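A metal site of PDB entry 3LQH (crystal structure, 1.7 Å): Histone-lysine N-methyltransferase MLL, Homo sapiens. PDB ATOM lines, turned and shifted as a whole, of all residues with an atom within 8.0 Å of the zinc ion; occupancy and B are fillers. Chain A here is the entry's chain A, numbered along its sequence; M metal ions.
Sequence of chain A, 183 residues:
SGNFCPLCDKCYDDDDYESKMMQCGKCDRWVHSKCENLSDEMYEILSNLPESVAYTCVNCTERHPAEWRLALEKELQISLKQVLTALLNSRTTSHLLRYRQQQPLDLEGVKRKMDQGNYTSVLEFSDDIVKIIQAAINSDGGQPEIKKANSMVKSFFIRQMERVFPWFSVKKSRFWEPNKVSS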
ATOM      1  N   PRO A   6     -24.193 -10.794  23.082  1.00  0.00           N
ATOM      2  CA  PRO A   6     -25.415 -11.450  23.577  1.00  0.00           C
ATOM      3  C   PRO A   6     -25.718 -11.334  25.059  1.00  0.00           C
ATOM      4  O   PRO A   6     -26.821 -11.672  25.503  1.00  0.00           O
ATOM      5  CB  PRO A   6     -25.230 -12.903  23.127  1.00  0.00           C
ATOM      6  CG  PRO A   6     -23.742 -13.070  23.202  1.00  0.00           C
ATOM      7  CD  PRO A   6     -23.228 -11.787  22.595  1.00  0.00           C
ATOM      8  N   GLN A  23     -14.007 -14.308  21.779  1.00  0.00           N
ATOM      9  CA  GLN A  23     -14.787 -14.795  20.661  1.00  0.00           C
ATOM     10  C   GLN A  23     -15.325 -16.223  20.823  1.00  0.00           C
ATOM     11  O   GLN A  23     -14.628 -17.119  21.297  1.00  0.00           O
ATOM     12  CB  GLN A  23     -13.945 -14.727  19.379  1.00  0.00           C
ATOM     13  CG  GLN A  23     -14.680 -15.113  18.110  1.00  0.00           C
ATOM     14  CD  GLN A  23     -13.824 -14.930  16.875  1.00  0.00           C
ATOM     15  OE1 GLN A  23     -12.675 -15.385  16.826  1.00  0.00           O
ATOM     16  NE2 GLN A  23     -14.366 -14.279  15.852  1.00  0.00           N
ATOM     17  N   CYS A  24     -16.574 -16.412  20.429  1.00  0.00           N
ATOM     18  CA  CYS A  24     -17.192 -17.718  20.489  1.00  0.00           C
ATOM     19  C   CYS A  24     -16.645 -18.523  19.323  1.00  0.00           C
ATOM     20  O   CYS A  24     -16.701 -18.081  18.172  1.00  0.00           O
ATOM     21  CB  CYS A  24     -18.710 -17.614  20.342  1.00  0.00           C
ATOM     22  SG  CYS A  24     -19.525 -19.215  20.170  1.00  0.00           S
ATOM     23  N   GLY A  25     -16.113 -19.708  19.618  1.00  0.00           N
ATOM     24  CA  GLY A  25     -15.536 -20.541  18.581  1.00  0.00           C
ATOM     25  C   GLY A  25     -16.532 -21.207  17.647  1.00  0.00           C
ATOM     26  O   GLY A  25     -16.147 -21.722  16.599  1.00  0.00           O
ATOM     27  N   LYS A  26     -17.811 -21.185  18.005  1.00  0.00           N
ATOM     28  CA  LYS A  26     -18.815 -21.797  17.154  1.00  0.00           C
ATOM     29  C   LYS A  26     -19.493 -20.834  16.192  1.00  0.00           C
ATOM     30  O   LYS A  26     -19.770 -21.193  15.048  1.00  0.00           O
ATOM     31  CB  LYS A  26     -19.872 -22.498  18.012  1.00  0.00           C
ATOM     32  CG  LYS A  26     -19.325 -23.640  18.848  1.00  0.00           C
ATOM     33  CD  LYS A  26     -20.448 -24.490  19.425  1.00  0.00           C
ATOM     34  CE  LYS A  26     -19.890 -25.587  20.323  1.00  0.00           C
ATOM     35  NZ  LYS A  26     -18.854 -26.397  19.615  1.00  0.00           N
ATOM     36  N   CYS A  27     -19.737 -19.592  16.629  1.00  0.00           N
ATOM     37  CA  CYS A  27     -20.407 -18.629  15.761  1.00  0.00           C
ATOM     38  C   CYS A  27     -19.612 -17.365  15.437  1.00  0.00           C
ATOM     39  O   CYS A  27     -20.096 -16.481  14.735  1.00  0.00           O
ATOM     40  CB  CYS A  27     -21.752 -18.224  16.370  1.00  0.00           C
ATOM     41  SG  CYS A  27     -21.617 -17.101  17.777  1.00  0.00           S
ATOM     42  N   ASP A  28     -18.395 -17.284  15.967  1.00  0.00           N
ATOM     43  CA  ASP A  28     -17.510 -16.132  15.751  1.00  0.00           C
ATOM     44  C   ASP A  28     -17.984 -14.793  16.318  1.00  0.00           C
ATOM     45  O   ASP A  28     -17.360 -13.762  16.044  1.00  0.00           O
ATOM     46  CB  ASP A  28     -17.201 -15.978  14.251  1.00  0.00           C
ATOM     47  CG  ASP A  28     -16.184 -16.997  13.751  1.00  0.00           C
ATOM     48  OD1 ASP A  28     -15.682 -17.781  14.582  1.00  0.00           O
ATOM     49  OD2 ASP A  28     -15.889 -17.001  12.542  1.00  0.00           O
ATOM     50  N   ARG A  29     -19.056 -14.802  17.100  1.00  0.00           N
ATOM     51  CA  ARG A  29     -19.541 -13.568  17.706  1.00  0.00           C
ATOM     52  C   ARG A  29     -18.648 -13.252  18.922  1.00  0.00           C
ATOM     53  O   ARG A  29     -18.031 -14.151  19.481  1.00  0.00           O
ATOM     54  CB  ARG A  29     -20.991 -13.718  18.187  1.00  0.00           C
ATOM     55  CG  ARG A  29     -22.012 -13.966  17.079  1.00  0.00           C
ATOM     56  CD  ARG A  29     -22.002 -12.861  16.027  1.00  0.00           C
ATOM     57  NE  ARG A  29     -23.183 -12.936  15.166  1.00  0.00           N
ATOM     58  CZ  ARG A  29     -23.329 -12.235  14.042  1.00  0.00           C
ATOM     59  NH1 ARG A  29     -24.440 -12.356  13.325  1.00  0.00           N
ATOM     60  NH2 ARG A  29     -22.373 -11.422  13.630  1.00  0.00           N
ATOM     61  N   TRP A  30     -18.598 -11.994  19.323  1.00  0.00           N
ATOM     62  CA  TRP A  30     -17.776 -11.577  20.455  1.00  0.00           C
ATOM     63  C   TRP A  30     -18.609 -11.238  21.687  1.00  0.00           C
ATOM     64  O   TRP A  30     -19.756 -10.803  21.572  1.00  0.00           O
ATOM     65  CB  TRP A  30     -16.898 -10.390  20.071  1.00  0.00           C
ATOM     66  CG  TRP A  30     -15.869 -10.738  19.040  1.00  0.00           C
ATOM     67  CD1 TRP A  30     -16.076 -10.889  17.692  1.00  0.00           C
ATOM     68  CD2 TRP A  30     -14.497 -11.059  19.282  1.00  0.00           C
ATOM     69  NE1 TRP A  30     -14.901 -11.277  17.075  1.00  0.00           N
ATOM     70  CE2 TRP A  30     -13.917 -11.386  18.027  1.00  0.00           C
ATOM     71  CE3 TRP A  30     -13.691 -11.100  20.425  1.00  0.00           C
ATOM     72  CZ2 TRP A  30     -12.579 -11.747  17.895  1.00  0.00           C
ATOM     73  CZ3 TRP A  30     -12.354 -11.461  20.293  1.00  0.00           C
ATOM     74  CH2 TRP A  30     -11.814 -11.778  19.038  1.00  0.00           C
ATOM     75  N   VAL A  31     -18.028 -11.460  22.864  1.00  0.00           N
ATOM     76  CA  VAL A  31     -18.693 -11.215  24.135  1.00  0.00           C
ATOM     77  C   VAL A  31     -17.787 -10.409  25.079  1.00  0.00           C
ATOM     78  O   VAL A  31     -16.603 -10.722  25.215  1.00  0.00           O
ATOM     79  CB  VAL A  31     -19.040 -12.559  24.827  1.00  0.00           C
ATOM     80  CG1 VAL A  31     -19.720 -12.317  26.158  1.00  0.00           C
ATOM     81  CG2 VAL A  31     -19.911 -13.400  23.903  1.00  0.00           C
ATOM     82  N   TYR A  55     -14.082 -21.239  24.222  1.00  0.00           N
ATOM     83  CA  TYR A  55     -15.219 -20.478  24.715  1.00  0.00           C
ATOM     84  C   TYR A  55     -16.395 -20.560  23.747  1.00  0.00           C
ATOM     85  O   TYR A  55     -16.227 -20.580  22.527  1.00  0.00           O
ATOM     86  CB  TYR A  55     -14.841 -19.002  24.900  1.00  0.00           C
ATOM     87  CG  TYR A  55     -15.991 -18.112  25.307  1.00  0.00           C
ATOM     88  CD1 TYR A  55     -16.497 -18.140  26.609  1.00  0.00           C
ATOM     89  CD2 TYR A  55     -16.613 -17.279  24.385  1.00  0.00           C
ATOM     90  CE1 TYR A  55     -17.600 -17.355  26.978  1.00  0.00           C
ATOM     91  CE2 TYR A  55     -17.715 -16.488  24.739  1.00  0.00           C
ATOM     92  CZ  TYR A  55     -18.202 -16.532  26.036  1.00  0.00           C
ATOM     93  OH  TYR A  55     -19.293 -15.784  26.392  1.00  0.00           O
ATOM     94  N   THR A  56     -17.603 -20.644  24.306  1.00  0.00           N
ATOM     95  CA  THR A  56     -18.823 -20.672  23.517  1.00  0.00           C
ATOM     96  C   THR A  56     -19.789 -19.685  24.152  1.00  0.00           C
ATOM     97  O   THR A  56     -19.889 -19.629  25.373  1.00  0.00           O
ATOM     98  CB  THR A  56     -19.467 -22.079  23.486  1.00  0.00           C
ATOM     99  OG1 THR A  56     -19.751 -22.520  24.825  1.00  0.00           O
ATOM    100  CG2 THR A  56     -18.540 -23.074  22.819  1.00  0.00           C
ATOM    101  N   CYS A  57     -20.472 -18.899  23.325  1.00  0.00           N
ATOM    102  CA  CYS A  57     -21.409 -17.913  23.856  1.00  0.00           C
ATOM    103  C   CYS A  57     -22.707 -18.581  24.315  1.00  0.00           C
ATOM    104  O   CYS A  57     -22.921 -19.767  24.090  1.00  0.00           O
ATOM    105  CB  CYS A  57     -21.728 -16.846  22.804  1.00  0.00           C
ATOM    106  SG  CYS A  57     -22.849 -17.384  21.493  1.00  0.00           S
ATOM    107  N   VAL A  58     -23.574 -17.788  24.944  1.00  0.00           N
ATOM    108  CA  VAL A  58     -24.836 -18.304  25.453  1.00  0.00           C
ATOM    109  C   VAL A  58     -25.696 -18.974  24.373  1.00  0.00           C
ATOM    110  O   VAL A  58     -26.405 -19.938  24.666  1.00  0.00           O
ATOM    111  CB  VAL A  58     -25.651 -17.177  26.119  1.00  0.00           C
ATOM    112  CG1 VAL A  58     -25.989 -16.098  25.101  1.00  0.00           C
ATOM    113  CG2 VAL A  58     -26.913 -17.760  26.744  1.00  0.00           C
ATOM    114  N   ASN A  59     -25.625 -18.487  23.146  1.00  0.00           N
ATOM    115  CA  ASN A  59     -26.422 -19.047  22.059  1.00  0.00           C
ATOM    116  C   ASN A  59     -25.862 -20.361  21.503  1.00  0.00           C
ATOM    117  O   ASN A  59     -26.573 -21.090  20.805  1.00  0.00           O
ATOM    118  CB  ASN A  59     -26.555 -18.048  20.909  1.00  0.00           C
ATOM    119  CG  ASN A  59     -27.299 -16.798  21.325  1.00  0.00           C
ATOM    120  OD1 ASN A  59     -28.402 -16.866  21.874  1.00  0.00           O
ATOM    121  ND2 ASN A  59     -26.708 -15.630  21.058  1.00  0.00           N
ATOM    122  N   CYS A  60     -24.607 -20.659  21.812  1.00  0.00           N
ATOM    123  CA  CYS A  60     -23.976 -21.860  21.312  1.00  0.00           C
ATOM    124  C   CYS A  60     -23.649 -22.867  22.401  1.00  0.00           C
ATOM    125  O   CYS A  60     -23.151 -23.963  22.118  1.00  0.00           O
ATOM    126  CB  CYS A  60     -22.711 -21.502  20.549  1.00  0.00           C
ATOM    127  SG  CYS A  60     -23.011 -20.463  19.095  1.00  0.00           S
ATOM    128  N   THR A  61     -23.988 -22.530  23.588  1.00  0.00           N
ATOM    129  CA  THR A  61     -23.696 -23.407  24.699  1.00  0.00           C
ATOM    130  C   THR A  61     -24.894 -24.318  24.989  1.00  0.00           C
ATOM    131  O   THR A  61     -25.856 -23.945  25.320  1.00  0.00           O
ATOM    132  CB  THR A  61     -23.324 -22.564  25.966  1.00  0.00           C
ATOM    133  OG1 THR A  61     -22.137 -21.823  25.701  1.00  0.00           O
ATOM    134  CG2 THR A  61     -23.011 -23.448  27.115  1.00  0.00           C
HETATM  135 ZN    ZN M   1     -21.763 -18.496  19.673  1.00  0.00          ZN
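SG of Cys 57 sits close to N of Asn 59, 3.4 Å away.
The backbone carbonyl oxygen (O) of Arg 29 is in hydrogen-bond range of the backbone NH (N) of Cys 24, at 2.9 Å.
The side-chain sulfur of Cys 27 lies close to the backbone NH of Arg 29.
The side-chain sulfur (SG) of Cys 24 lies close to the backbone NH (N) of Lys 26 (3.4 Å).
OG1 of Thr 61 sits at hydrogen-bond distance from O of Cys 57 (2.7 Å).
The zinc ion is bound by the side-chain sulfur of Cys 27 (2.4 Å), the side-chain sulfur of Cys 57 (2.4 Å), the side-chain sulfur of Cys 60 (2.4 Å) and the side-chain sulfur of Cys 24 (2.4 Å).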
